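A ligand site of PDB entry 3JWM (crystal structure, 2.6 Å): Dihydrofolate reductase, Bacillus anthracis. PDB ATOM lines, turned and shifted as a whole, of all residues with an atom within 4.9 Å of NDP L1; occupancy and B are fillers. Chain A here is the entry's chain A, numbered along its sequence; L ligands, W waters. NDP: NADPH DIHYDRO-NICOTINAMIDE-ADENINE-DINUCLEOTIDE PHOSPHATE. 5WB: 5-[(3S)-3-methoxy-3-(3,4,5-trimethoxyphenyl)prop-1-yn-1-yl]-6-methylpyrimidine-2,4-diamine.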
ATOM      1  N   MET A  12     -22.003  26.096 -17.317  1.00  0.00           N
ATOM      2  CA  MET A  12     -20.618  26.352 -16.921  1.00  0.00           C
ATOM      3  C   MET A  12     -19.742  25.832 -18.056  1.00  0.00           C
ATOM      4  O   MET A  12     -19.737  24.645 -18.349  1.00  0.00           O
ATOM      5  CB  MET A  12     -20.295  25.661 -15.601  1.00  0.00           C
ATOM      6  CG  MET A  12     -18.833  25.743 -15.155  1.00  0.00           C
ATOM      7  SD  MET A  12     -18.186  27.421 -14.828  1.00  0.00           S
ATOM      8  CE  MET A  12     -19.059  27.855 -13.313  1.00  0.00           C
ATOM      9  N   VAL A  13     -19.023  26.752 -18.700  1.00  0.00           N
ATOM     10  CA  VAL A  13     -18.206  26.416 -19.864  1.00  0.00           C
ATOM     11  C   VAL A  13     -16.996  27.335 -20.014  1.00  0.00           C
ATOM     12  O   VAL A  13     -17.052  28.519 -19.662  1.00  0.00           O
ATOM     13  CB  VAL A  13     -19.043  26.407 -21.186  1.00  0.00           C
ATOM     14  CG1 VAL A  13     -19.517  27.804 -21.586  1.00  0.00           C
ATOM     15  CG2 VAL A  13     -18.270  25.760 -22.328  1.00  0.00           C
ATOM     16  N   ALA A  14     -15.901  26.771 -20.515  1.00  0.00           N
ATOM     17  CA  ALA A  14     -14.741  27.530 -20.958  1.00  0.00           C
ATOM     18  C   ALA A  14     -14.551  27.312 -22.463  1.00  0.00           C
ATOM     19  O   ALA A  14     -14.543  26.166 -22.934  1.00  0.00           O
ATOM     20  CB  ALA A  14     -13.500  27.112 -20.190  1.00  0.00           C
ATOM     21  N   ILE A  21     -14.085  23.895 -27.329  1.00  0.00           N
ATOM     22  CA  ILE A  21     -14.106  23.471 -25.929  1.00  0.00           C
ATOM     23  C   ILE A  21     -13.328  22.153 -25.725  1.00  0.00           C
ATOM     24  O   ILE A  21     -13.005  21.794 -24.592  1.00  0.00           O
ATOM     25  CB  ILE A  21     -15.547  23.310 -25.350  1.00  0.00           C
ATOM     26  CG1 ILE A  21     -16.292  22.145 -26.023  1.00  0.00           C
ATOM     27  CG2 ILE A  21     -16.320  24.643 -25.446  1.00  0.00           C
ATOM     28  CD1 ILE A  21     -17.587  21.759 -25.349  1.00  0.00           C
ATOM     29  N   GLY A  22     -13.035  21.454 -26.825  1.00  0.00           N
ATOM     30  CA  GLY A  22     -12.423  20.133 -26.732  1.00  0.00           C
ATOM     31  C   GLY A  22     -11.618  19.647 -27.921  1.00  0.00           C
ATOM     32  O   GLY A  22     -11.865  20.037 -29.065  1.00  0.00           O
ATOM     33  N   LYS A  23     -10.658  18.783 -27.630  1.00  0.00           N
ATOM     34  CA  LYS A  23      -9.793  18.178 -28.629  1.00  0.00           C
ATOM     35  C   LYS A  23      -9.459  16.756 -28.192  1.00  0.00           C
ATOM     36  O   LYS A  23      -8.998  16.545 -27.068  1.00  0.00           O
ATOM     37  CB  LYS A  23      -8.494  18.971 -28.768  1.00  0.00           C
ATOM     38  CG  LYS A  23      -7.596  18.485 -29.900  1.00  0.00           C
ATOM     39  CD  LYS A  23      -6.133  18.856 -29.667  1.00  0.00           C
ATOM     40  CE  LYS A  23      -5.246  18.222 -30.752  1.00  0.00           C
ATOM     41  NZ  LYS A  23      -3.939  18.923 -30.875  1.00  0.00           N
ATOM     42  N   ASN A  25     -11.322  14.354 -27.198  1.00  0.00           N
ATOM     43  CA  ASN A  25     -12.042  14.007 -25.963  1.00  0.00           C
ATOM     44  C   ASN A  25     -11.368  14.497 -24.673  1.00  0.00           C
ATOM     45  O   ASN A  25     -11.507  13.896 -23.592  1.00  0.00           O
ATOM     46  CB  ASN A  25     -12.317  12.502 -25.905  1.00  0.00           C
ATOM     47  CG  ASN A  25     -13.464  12.141 -24.990  1.00  0.00           C
ATOM     48  OD1 ASN A  25     -14.441  12.894 -24.862  1.00  0.00           O
ATOM     49  ND2 ASN A  25     -13.373  10.978 -24.346  1.00  0.00           N
ATOM     50  N   ASN A  26     -10.632  15.599 -24.800  1.00  0.00           N
ATOM     51  CA  ASN A  26      -9.958  16.234 -23.683  1.00  0.00           C
ATOM     52  C   ASN A  26     -10.021  17.752 -23.784  1.00  0.00           C
ATOM     53  O   ASN A  26     -10.500  18.307 -24.778  1.00  0.00           O
ATOM     54  CB  ASN A  26      -8.506  15.757 -23.569  1.00  0.00           C
ATOM     55  CG  ASN A  26      -8.268  14.893 -22.330  1.00  0.00           C
ATOM     56  OD1 ASN A  26      -8.104  13.677 -22.426  1.00  0.00           O
ATOM     57  ND2 ASN A  26      -8.264  15.533 -21.153  1.00  0.00           N
ATOM     58  N   LEU A  27      -9.557  18.415 -22.732  1.00  0.00           N
ATOM     59  CA  LEU A  27      -9.408  19.859 -22.675  1.00  0.00           C
ATOM     60  C   LEU A  27      -8.133  20.232 -23.422  1.00  0.00           C
ATOM     61  O   LEU A  27      -7.097  19.593 -23.224  1.00  0.00           O
ATOM     62  CB  LEU A  27      -9.279  20.252 -21.218  1.00  0.00           C
ATOM     63  CG  LEU A  27     -10.130  21.328 -20.532  1.00  0.00           C
ATOM     64  CD1 LEU A  27     -11.500  21.546 -21.190  1.00  0.00           C
ATOM     65  CD2 LEU A  27     -10.282  20.912 -19.071  1.00  0.00           C
ATOM     66  N   TRP A  29      -6.375  22.972 -23.117  1.00  0.00           N
ATOM     67  CA  TRP A  29      -5.526  23.880 -22.355  1.00  0.00           C
ATOM     68  C   TRP A  29      -5.415  23.436 -20.902  1.00  0.00           C
ATOM     69  O   TRP A  29      -6.315  22.786 -20.368  1.00  0.00           O
ATOM     70  CB  TRP A  29      -6.062  25.300 -22.417  1.00  0.00           C
ATOM     71  CG  TRP A  29      -7.533  25.383 -22.075  1.00  0.00           C
ATOM     72  CD1 TRP A  29      -8.086  25.401 -20.837  1.00  0.00           C
ATOM     73  CD2 TRP A  29      -8.619  25.446 -23.009  1.00  0.00           C
ATOM     74  NE1 TRP A  29      -9.449  25.480 -20.919  1.00  0.00           N
ATOM     75  CE2 TRP A  29      -9.813  25.502 -22.250  1.00  0.00           C
ATOM     76  CE3 TRP A  29      -8.709  25.471 -24.398  1.00  0.00           C
ATOM     77  CZ2 TRP A  29     -11.074  25.574 -22.844  1.00  0.00           C
ATOM     78  CZ3 TRP A  29      -9.979  25.544 -24.994  1.00  0.00           C
ATOM     79  CH2 TRP A  29     -11.139  25.586 -24.211  1.00  0.00           C
ATOM     80  N   GLY A  50     -22.322  15.149 -19.671  1.00  0.00           N
ATOM     81  CA  GLY A  50     -22.512  14.109 -20.685  1.00  0.00           C
ATOM     82  C   GLY A  50     -21.663  12.894 -20.364  1.00  0.00           C
ATOM     83  O   GLY A  50     -20.608  13.026 -19.758  1.00  0.00           O
ATOM     84  N   ARG A  51     -22.114  11.716 -20.788  1.00  0.00           N
ATOM     85  CA  ARG A  51     -21.393  10.466 -20.506  1.00  0.00           C
ATOM     86  C   ARG A  51     -19.918  10.546 -20.900  1.00  0.00           C
ATOM     87  O   ARG A  51     -19.043  10.198 -20.096  1.00  0.00           O
ATOM     88  CB  ARG A  51     -22.101   9.275 -21.175  1.00  0.00           C
ATOM     89  CG  ARG A  51     -21.777   7.901 -20.589  1.00  0.00           C
ATOM     90  CD  ARG A  51     -20.661   7.203 -21.363  1.00  0.00           C
ATOM     91  NE  ARG A  51     -20.968   7.131 -22.788  1.00  0.00           N
ATOM     92  CZ  ARG A  51     -20.067   7.044 -23.764  1.00  0.00           C
ATOM     93  NH1 ARG A  51     -18.772   7.025 -23.478  1.00  0.00           N
ATOM     94  NH2 ARG A  51     -20.459   6.998 -25.024  1.00  0.00           N
ATOM     95  N   LYS A  52     -19.626  11.041 -22.111  1.00  0.00           N
ATOM     96  CA  LYS A  52     -18.255  11.192 -22.580  1.00  0.00           C
ATOM     97  C   LYS A  52     -17.460  12.154 -21.698  1.00  0.00           C
ATOM     98  O   LYS A  52     -16.383  11.792 -21.208  1.00  0.00           O
ATOM     99  CB  LYS A  52     -18.183  11.593 -24.056  1.00  0.00           C
ATOM    100  CG  LYS A  52     -18.392  10.441 -25.024  1.00  0.00           C
ATOM    101  CD  LYS A  52     -17.686  10.713 -26.346  1.00  0.00           C
ATOM    102  CE  LYS A  52     -18.409  10.040 -27.497  1.00  0.00           C
ATOM    103  NZ  LYS A  52     -17.722  10.227 -28.816  1.00  0.00           N
ATOM    104  N   ASN A  53     -17.980  13.354 -21.487  1.00  0.00           N
ATOM    105  CA  ASN A  53     -17.364  14.268 -20.531  1.00  0.00           C
ATOM    106  C   ASN A  53     -16.957  13.527 -19.261  1.00  0.00           C
ATOM    107  O   ASN A  53     -15.784  13.575 -18.876  1.00  0.00           O
ATOM    108  CB  ASN A  53     -18.272  15.458 -20.195  1.00  0.00           C
ATOM    109  CG  ASN A  53     -17.639  16.424 -19.191  1.00  0.00           C
ATOM    110  OD1 ASN A  53     -16.434  16.402 -18.975  1.00  0.00           O
ATOM    111  ND2 ASN A  53     -18.457  17.289 -18.583  1.00  0.00           N
ATOM    112  N   VAL A  69     -25.549  12.073 -17.997  1.00  0.00           N
ATOM    113  CA  VAL A  69     -26.585  11.957 -19.022  1.00  0.00           C
ATOM    114  C   VAL A  69     -26.151  11.018 -20.134  1.00  0.00           C
ATOM    115  O   VAL A  69     -25.145  11.260 -20.807  1.00  0.00           O
ATOM    116  CB  VAL A  69     -27.014  13.341 -19.588  1.00  0.00           C
ATOM    117  CG1 VAL A  69     -28.123  13.196 -20.624  1.00  0.00           C
ATOM    118  CG2 VAL A  69     -27.462  14.253 -18.472  1.00  0.00           C
ATOM    119  N   THR A  70     -26.918   9.937 -20.302  1.00  0.00           N
ATOM    120  CA  THR A  70     -26.612   8.874 -21.257  1.00  0.00           C
ATOM    121  C   THR A  70     -27.914   8.285 -21.797  1.00  0.00           C
ATOM    122  O   THR A  70     -28.963   8.384 -21.159  1.00  0.00           O
ATOM    123  CB  THR A  70     -25.753   7.763 -20.615  1.00  0.00           C
ATOM    124  OG1 THR A  70     -25.585   6.681 -21.540  1.00  0.00           O
ATOM    125  CG2 THR A  70     -26.386   7.233 -19.332  1.00  0.00           C
ATOM    126  N   ARG A  71     -27.844   7.670 -22.978  1.00  0.00           N
ATOM    127  CA  ARG A  71     -28.996   6.952 -23.518  1.00  0.00           C
ATOM    128  C   ARG A  71     -29.029   5.517 -23.025  1.00  0.00           C
ATOM    129  O   ARG A  71     -30.038   4.839 -23.160  1.00  0.00           O
ATOM    130  CB  ARG A  71     -29.003   6.972 -25.048  1.00  0.00           C
ATOM    131  CG  ARG A  71     -29.403   8.306 -25.628  1.00  0.00           C
ATOM    132  CD  ARG A  71     -29.533   8.253 -27.135  1.00  0.00           C
ATOM    133  NE  ARG A  71     -29.701   9.590 -27.699  1.00  0.00           N
ATOM    134  CZ  ARG A  71     -28.700  10.383 -28.083  1.00  0.00           C
ATOM    135  NH1 ARG A  71     -27.433   9.970 -27.980  1.00  0.00           N
ATOM    136  NH2 ARG A  71     -28.954  11.587 -28.569  1.00  0.00           N
ATOM    137  N   ASN A  72     -27.913   5.074 -22.445  1.00  0.00           N
ATOM    138  CA  ASN A  72     -27.734   3.713 -21.955  1.00  0.00           C
ATOM    139  C   ASN A  72     -28.561   3.458 -20.698  1.00  0.00           C
ATOM    140  O   ASN A  72     -28.283   4.003 -19.630  1.00  0.00           O
ATOM    141  CB  ASN A  72     -26.249   3.509 -21.636  1.00  0.00           C
ATOM    142  CG  ASN A  72     -25.845   2.049 -21.532  1.00  0.00           C
ATOM    143  OD1 ASN A  72     -24.726   1.692 -21.873  1.00  0.00           O
ATOM    144  ND2 ASN A  72     -26.753   1.196 -21.069  1.00  0.00           N
ATOM    145  N   HIS A  84     -31.396  10.024 -18.274  1.00  0.00           N
ATOM    146  CA  HIS A  84     -31.413   9.620 -19.677  1.00  0.00           C
ATOM    147  C   HIS A  84     -32.107  10.638 -20.583  1.00  0.00           C
ATOM    148  O   HIS A  84     -32.228  10.421 -21.794  1.00  0.00           O
ATOM    149  CB  HIS A  84     -32.040   8.233 -19.827  1.00  0.00           C
ATOM    150  CG  HIS A  84     -31.473   7.217 -18.888  1.00  0.00           C
ATOM    151  ND1 HIS A  84     -31.908   7.089 -17.585  1.00  0.00           N
ATOM    152  CD2 HIS A  84     -30.509   6.284 -19.050  1.00  0.00           C
ATOM    153  CE1 HIS A  84     -31.232   6.124 -16.987  1.00  0.00           C
ATOM    154  NE2 HIS A  84     -30.378   5.622 -17.851  1.00  0.00           N
ATOM    155  N   SER A  85     -32.522  11.753 -19.992  1.00  0.00           N
ATOM    156  CA  SER A  85     -33.242  12.798 -20.717  1.00  0.00           C
ATOM    157  C   SER A  85     -33.206  14.122 -19.967  1.00  0.00           C
ATOM    158  O   SER A  85     -32.842  14.179 -18.780  1.00  0.00           O
ATOM    159  CB  SER A  85     -34.710  12.378 -20.947  1.00  0.00           C
ATOM    160  OG  SER A  85     -35.415  12.291 -19.712  1.00  0.00           O
ATOM    161  N   PHE A 102     -22.597  21.211 -17.398  1.00  0.00           N
ATOM    162  CA  PHE A 102     -21.156  21.182 -17.207  1.00  0.00           C
ATOM    163  C   PHE A 102     -20.404  20.609 -18.427  1.00  0.00           C
ATOM    164  O   PHE A 102     -19.182  20.474 -18.388  1.00  0.00           O
ATOM    165  CB  PHE A 102     -20.875  20.342 -15.968  1.00  0.00           C
ATOM    166  CG  PHE A 102     -19.575  20.669 -15.256  1.00  0.00           C
ATOM    167  CD1 PHE A 102     -19.395  21.896 -14.632  1.00  0.00           C
ATOM    168  CD2 PHE A 102     -18.569  19.716 -15.180  1.00  0.00           C
ATOM    169  CE1 PHE A 102     -18.210  22.190 -13.980  1.00  0.00           C
ATOM    170  CE2 PHE A 102     -17.386  19.996 -14.525  1.00  0.00           C
ATOM    171  CZ  PHE A 102     -17.201  21.247 -13.921  1.00  0.00           C
ATOM    172  N   GLY A 103     -21.137  20.290 -19.502  1.00  0.00           N
ATOM    173  CA  GLY A 103     -20.544  19.818 -20.753  1.00  0.00           C
ATOM    174  C   GLY A 103     -20.611  18.314 -20.974  1.00  0.00           C
ATOM    175  O   GLY A 103     -21.027  17.574 -20.089  1.00  0.00           O
ATOM    176  N   GLY A 104     -20.201  17.836 -22.161  1.00  0.00           N
ATOM    177  CA  GLY A 104     -19.684  18.665 -23.244  1.00  0.00           C
ATOM    178  C   GLY A 104     -20.743  19.180 -24.200  1.00  0.00           C
ATOM    179  O   GLY A 104     -21.874  19.431 -23.784  1.00  0.00           O
ATOM    180  N   ALA A 105     -20.373  19.323 -25.472  1.00  0.00           N
ATOM    181  CA  ALA A 105     -21.206  19.946 -26.502  1.00  0.00           C
ATOM    182  C   ALA A 105     -22.597  19.326 -26.696  1.00  0.00           C
ATOM    183  O   ALA A 105     -23.591  20.063 -26.785  1.00  0.00           O
ATOM    184  CB  ALA A 105     -20.451  19.984 -27.828  1.00  0.00           C
ATOM    185  N   GLN A 106     -22.669  18.005 -26.777  1.00  0.00           N
ATOM    186  CA  GLN A 106     -23.962  17.325 -26.987  1.00  0.00           C
ATOM    187  C   GLN A 106     -24.945  17.660 -25.861  1.00  0.00           C
ATOM    188  O   GLN A 106     -26.126  17.878 -26.104  1.00  0.00           O
ATOM    189  CB  GLN A 106     -23.785  15.807 -27.091  1.00  0.00           C
ATOM    190  CG  GLN A 106     -23.037  15.342 -28.352  1.00  0.00           C
ATOM    191  CD  GLN A 106     -23.107  13.827 -28.556  1.00  0.00           C
ATOM    192  OE1 GLN A 106     -22.096  13.172 -28.784  1.00  0.00           O
ATOM    193  NE2 GLN A 106     -24.307  13.269 -28.452  1.00  0.00           N
ATOM    194  N   ILE A 107     -24.425  17.713 -24.629  1.00  0.00           N
ATOM    195  CA  ILE A 107     -25.202  18.054 -23.453  1.00  0.00           C
ATOM    196  C   ILE A 107     -25.503  19.551 -23.354  1.00  0.00           C
ATOM    197  O   ILE A 107     -26.572  19.934 -22.866  1.00  0.00           O
ATOM    198  CB  ILE A 107     -24.576  17.423 -22.149  1.00  0.00           C
ATOM    199  CG1 ILE A 107     -25.402  16.218 -21.710  1.00  0.00           C
ATOM    200  CG2 ILE A 107     -24.441  18.418 -21.007  1.00  0.00           C
ATOM    201  CD1 ILE A 107     -25.477  15.076 -22.750  1.00  0.00           C
ATOM    202  N   TYR A 108     -24.600  20.399 -23.845  1.00  0.00           N
ATOM    203  CA  TYR A 108     -24.890  21.839 -23.973  1.00  0.00           C
ATOM    204  C   TYR A 108     -26.021  22.078 -24.962  1.00  0.00           C
ATOM    205  O   TYR A 108     -26.955  22.810 -24.669  1.00  0.00           O
ATOM    206  CB  TYR A 108     -23.661  22.651 -24.367  1.00  0.00           C
ATOM    207  CG  TYR A 108     -22.587  22.809 -23.296  1.00  0.00           C
ATOM    208  CD1 TYR A 108     -22.923  23.117 -21.971  1.00  0.00           C
ATOM    209  CD2 TYR A 108     -21.245  22.680 -23.623  1.00  0.00           C
ATOM    210  CE1 TYR A 108     -21.936  23.256 -21.003  1.00  0.00           C
ATOM    211  CE2 TYR A 108     -20.254  22.830 -22.671  1.00  0.00           C
ATOM    212  CZ  TYR A 108     -20.610  23.123 -21.360  1.00  0.00           C
ATOM    213  OH  TYR A 108     -19.609  23.264 -20.412  1.00  0.00           O
ATOM    214  N   LEU A 110     -28.320  19.954 -25.779  1.00  0.00           N
ATOM    215  CA  LEU A 110     -29.533  19.363 -25.230  1.00  0.00           C
ATOM    216  C   LEU A 110     -30.273  20.317 -24.295  1.00  0.00           C
ATOM    217  O   LEU A 110     -31.503  20.434 -24.360  1.00  0.00           O
ATOM    218  CB  LEU A 110     -29.194  18.045 -24.508  1.00  0.00           C
ATOM    219  CG  LEU A 110     -30.371  17.155 -24.103  1.00  0.00           C
ATOM    220  CD1 LEU A 110     -31.173  16.718 -25.328  1.00  0.00           C
ATOM    221  CD2 LEU A 110     -29.881  15.941 -23.319  1.00  0.00           C
ATOM    222  N   THR A 131     -14.381  19.928 -30.882  1.00  0.00           N
ATOM    223  CA  THR A 131     -15.640  20.049 -30.132  1.00  0.00           C
ATOM    224  C   THR A 131     -15.944  21.515 -29.777  1.00  0.00           C
ATOM    225  O   THR A 131     -15.067  22.242 -29.291  1.00  0.00           O
ATOM    226  CB  THR A 131     -15.621  19.151 -28.878  1.00  0.00           C
ATOM    227  OG1 THR A 131     -15.178  17.847 -29.245  1.00  0.00           O
ATOM    228  CG2 THR A 131     -17.001  19.023 -28.277  1.00  0.00           C
HETATM  229  PA  NDP L   1     -20.686  14.867 -24.076  1.00  0.00           P
HETATM  230  O1A NDP L   1     -21.648  15.908 -24.497  1.00  0.00           O
HETATM  231  O2A NDP L   1     -20.039  15.179 -22.785  1.00  0.00           O
HETATM  232  O5B NDP L   1     -21.365  13.419 -23.999  1.00  0.00           O
HETATM  233  C5B NDP L   1     -22.008  12.886 -25.129  1.00  0.00           C
HETATM  234  C4B NDP L   1     -22.784  11.691 -24.612  1.00  0.00           C
HETATM  235  O4B NDP L   1     -23.870  12.167 -23.840  1.00  0.00           O
HETATM  236  C3B NDP L   1     -23.399  10.812 -25.678  1.00  0.00           C
HETATM  237  O3B NDP L   1     -22.486   9.859 -26.164  1.00  0.00           O
HETATM  238  C2B NDP L   1     -24.539  10.186 -24.905  1.00  0.00           C
HETATM  239  O2B NDP L   1     -24.061   9.181 -24.039  1.00  0.00           O
HETATM  240  C1B NDP L   1     -24.983  11.315 -23.999  1.00  0.00           C
HETATM  241  N9A NDP L   1     -26.081  12.013 -24.666  1.00  0.00           N
HETATM  242  C8A NDP L   1     -25.994  12.927 -25.682  1.00  0.00           C
HETATM  243  N7A NDP L   1     -27.247  13.309 -26.017  1.00  0.00           N
HETATM  244  C5A NDP L   1     -28.127  12.653 -25.231  1.00  0.00           C
HETATM  245  C6A NDP L   1     -29.500  12.680 -25.156  1.00  0.00           C
HETATM  246  N6A NDP L   1     -30.190  13.462 -25.969  1.00  0.00           N
HETATM  247  N1A NDP L   1     -30.162  11.879 -24.232  1.00  0.00           N
HETATM  248  C2A NDP L   1     -29.430  11.080 -23.372  1.00  0.00           C
HETATM  249  N3A NDP L   1     -28.053  11.064 -23.464  1.00  0.00           N
HETATM  250  C4A NDP L   1     -27.417  11.834 -24.377  1.00  0.00           C
HETATM  251  O3  NDP L   1     -19.624  14.610 -25.269  1.00  0.00           O
HETATM  252  PN  NDP L   1     -18.971  15.616 -26.330  1.00  0.00           P
HETATM  253  O1N NDP L   1     -18.110  14.806 -27.231  1.00  0.00           O
HETATM  254  O2N NDP L   1     -20.052  16.451 -26.895  1.00  0.00           O
HETATM  255  O5D NDP L   1     -18.054  16.559 -25.398  1.00  0.00           O
HETATM  256  C5D NDP L   1     -16.844  16.073 -24.861  1.00  0.00           C
HETATM  257  C4D NDP L   1     -15.722  17.068 -25.114  1.00  0.00           C
HETATM  258  O4D NDP L   1     -16.028  18.358 -24.594  1.00  0.00           O
HETATM  259  C3D NDP L   1     -14.465  16.597 -24.413  1.00  0.00           C
HETATM  260  O3D NDP L   1     -13.379  16.881 -25.245  1.00  0.00           O
HETATM  261  C2D NDP L   1     -14.402  17.458 -23.155  1.00  0.00           C
HETATM  262  O2D NDP L   1     -13.077  17.679 -22.723  1.00  0.00           O
HETATM  263  C1D NDP L   1     -15.046  18.751 -23.635  1.00  0.00           C
HETATM  264  N1N NDP L   1     -15.608  19.532 -22.518  1.00  0.00           N
HETATM  265  C2N NDP L   1     -15.203  20.849 -22.425  1.00  0.00           C
HETATM  266  C3N NDP L   1     -15.663  21.682 -21.409  1.00  0.00           C
HETATM  267  C7N NDP L   1     -15.228  23.115 -21.369  1.00  0.00           C
HETATM  268  O7N NDP L   1     -15.916  24.026 -20.534  1.00  0.00           O
HETATM  269  N7N NDP L   1     -14.201  23.523 -22.136  1.00  0.00           N
HETATM  270  C4N NDP L   1     -16.555  21.155 -20.471  1.00  0.00           C
HETATM  271  C5N NDP L   1     -16.963  19.817 -20.566  1.00  0.00           C
HETATM  272  C6N NDP L   1     -16.478  19.005 -21.598  1.00  0.00           C
HETATM  273  P2B NDP L   1     -24.151   7.626 -24.406  1.00  0.00           P
HETATM  274  O1X NDP L   1     -25.576   7.282 -24.793  1.00  0.00           O
HETATM  275  O2X NDP L   1     -23.242   7.384 -25.587  1.00  0.00           O
HETATM  276  O3X NDP L   1     -23.675   6.838 -23.210  1.00  0.00           O
HETATM  277  N1  5WB L   2     -14.212  25.313 -17.200  1.00  0.00           N
HETATM  278  C2  5WB L   2     -15.399  25.910 -17.313  1.00  0.00           C
HETATM  279  N3  5WB L   2     -16.519  25.179 -17.421  1.00  0.00           N
HETATM  280  C4  5WB L   2     -16.484  23.840 -17.418  1.00  0.00           C
HETATM  281  C5  5WB L   2     -15.250  23.200 -17.311  1.00  0.00           C
HETATM  282  C6  5WB L   2     -14.097  23.981 -17.187  1.00  0.00           C
HETATM  283  C1A 5WB L   2     -12.730  20.508 -12.427  1.00  0.00           C
HETATM  284  C1B 5WB L   2     -10.691  16.278 -17.376  1.00  0.00           C
HETATM  285  C1C 5WB L   2     -11.154  16.746 -12.691  1.00  0.00           C
HETATM  286  C1D 5WB L   2     -13.675  19.207 -19.419  1.00  0.00           C
HETATM  287  C1E 5WB L   2     -12.702  23.345 -17.066  1.00  0.00           C
HETATM  288  N1F 5WB L   2     -15.457  27.239 -17.303  1.00  0.00           N
HETATM  289  N1G 5WB L   2     -17.591  23.127 -17.536  1.00  0.00           N
HETATM  290  C1H 5WB L   2     -15.183  21.778 -17.305  1.00  0.00           C
HETATM  291  C1I 5WB L   2     -15.095  20.571 -17.304  1.00  0.00           C
HETATM  292  C1J 5WB L   2     -13.965  19.102 -14.950  1.00  0.00           C
HETATM  293  C1K 5WB L   2     -12.642  18.147 -16.720  1.00  0.00           C
HETATM  294  O1N 5WB L   2     -13.109  19.138 -12.715  1.00  0.00           O
HETATM  295  O1O 5WB L   2     -10.474  17.212 -16.268  1.00  0.00           O
HETATM  296  O1P 5WB L   2     -10.819  17.900 -13.523  1.00  0.00           O
HETATM  297  O1Q 5WB L   2     -14.695  18.558 -18.646  1.00  0.00           O
HETATM  298  C1U 5WB L   2     -13.811  18.770 -16.294  1.00  0.00           C
HETATM  299  C1W 5WB L   2     -12.949  18.811 -14.031  1.00  0.00           C
HETATM  300  C1X 5WB L   2     -11.617  17.838 -15.810  1.00  0.00           C
HETATM  301  C1Y 5WB L   2     -11.781  18.180 -14.462  1.00  0.00           C
HETATM  302  C1Z 5WB L   2     -14.941  19.101 -17.298  1.00  0.00           C
HETATM  303  O   HOH W   1     -33.330  12.151 -24.674  1.00  0.00           O
HETATM  304  O   HOH W   2     -22.685  10.198 -28.968  1.00  0.00           O
HETATM  305  O   HOH W   3     -26.235   7.545 -27.313  1.00  0.00           O
HETATM  306  O   HOH W   4     -15.126  14.180 -27.053  1.00  0.00           O
HETATM  307  O   HOH W   5     -22.988   4.062 -22.481  1.00  0.00           O
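OG1 of Thr 70 sits at hydrogen-bond distance from O3X of NDP L1, at 2.5 Å.
O2A of NDP L1 is in hydrogen-bond range of N of Gly 104 (2.7 Å).
O7N of NDP L1 lies within hydrogen-bond range of N of Ala 14.
N7N of NDP L1 sits at hydrogen-bond distance from O of Ala 14 (2.8 Å).
O3X of NDP L1 lies within salt-bridge range of NE of Arg 51 (2.8 Å).
An oxygen (O1X) of NDP L1 is in hydrogen-bond range of the backbone NH of Arg 71 (2.9 Å).
N of Asn 53 is in hydrogen-bond range of O2A of NDP L1 (3.0 Å).
The backbone NH (N) of Gln 106 lies within hydrogen-bond range of an oxygen (O2N) of NDP L1, 3.0 Å away.
The backbone NH (N) of Asn 26 is in hydrogen-bond range of an oxygen (O3D) of NDP L1, 3.1 Å away.
O of Asn 26 lies within hydrogen-bond range of O3D of NDP L1 (3.2 Å).
The backbone NH (N) of Ala 105 sits at hydrogen-bond distance from an oxygen (O2N) of NDP L1, at 3.2 Å.
O of Ile 21 lies close to N7N of NDP L1 (3.2 Å).
An oxygen (O1A) of NDP L1 lies within hydrogen-bond range of the backbone NH (N) of Ile 107, 3.3 Å away.
The backbone NH (N) of Lys 52 lies within hydrogen-bond range of an oxygen (O5B) of NDP L1 (3.5 Å).
An oxygen (O1Q) of 5WB L2 sits close to the side-chain amide oxygen of Asn 53 (2.8 Å).
The backbone carbonyl oxygen of Phe 102 is in hydrogen-bond range of a nitrogen (N1G) of 5WB L2.
A nitrogen (N3) of 5WB L2 lies close to the backbone NH (N) of Val 13, at 3.2 Å.
The backbone carbonyl oxygen of Val 13 lies close to a nitrogen (N1F) of 5WB L2 (3.1 Å).
The backbone carbonyl oxygen (O) of Met 12 is in hydrogen-bond range of a nitrogen (N1G) of 5WB L2.
A nitrogen (N1F) of 5WB L2 is in hydrogen-bond range of the side-chain sulfur of Met 12, at 3.7 Å.
OG1 of Thr 70 is in hydrogen-bond range of N of Asn 72.
The backbone NH of Arg 51 sits at hydrogen-bond distance from the backbone carbonyl oxygen of Val 69, 3.1 Å away.
The side-chain amide nitrogen of Asn 53 is in hydrogen-bond range of the backbone carbonyl oxygen of Gly 103, at 3.0 Å.
The side-chain hydroxyl (OH) of Tyr 108 sits close to the backbone carbonyl oxygen (O) of Phe 102 (3.5 Å).
NE2 of His 84 lies within hydrogen-bond range of O of Asn 72.
The backbone NH (N) of Gly 50 sits at hydrogen-bond distance from the backbone carbonyl oxygen (O) of Gly 103 (2.8 Å).
OH of Tyr 108 lies close to N of Gly 103, at 3.5 Å.
O of Met 12 sits at hydrogen-bond distance from OH of Tyr 108, at 2.5 Å.
O of Val 69 lies close to O4B of NDP L1 (3.4 Å).
Merely in contact with NDP L1: Asn 25 (3.2 Å), Phe 102 (3.2 Å), His 84 (3.3 Å), Val 13 (3.4 Å), Gly 50 (3.4 Å), Leu 110 (3.5 Å), Leu 27 (3.5 Å), Gly 103 (3.6 Å), Gly 22 (3.7 Å), Tyr 108 (3.7 Å), Trp 29 (3.8 Å), Thr 131 (3.9 Å) and Asn 72 (3.98 Å).
Hydrophobic or aromatic side chains that line NDP L1: Val 13, Ala 14, Ile 21, Leu 27, Trp 29, Val 69, Ala 105, Ile 107 and Leu 110.
Water W3 lies within hydrogen-bond range of O1X of NDP L1 (2.6 Å) and NH1 of Arg 71 (2.8 Å).
Water W2 lies within hydrogen-bond range of an oxygen (O3B) of NDP L1 and the side-chain amide oxygen (OE1) of Gln 106.
Water W5 lies within hydrogen-bond range of an oxygen (O3X) of NDP L1 and the side-chain amide oxygen (OD1) of Asn 72.
Water W4 bridges the side-chain amide oxygen (OD1) of Asn 25 (2.6 Å) and an oxygen (O1N) of NDP L1 (3.1 Å).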
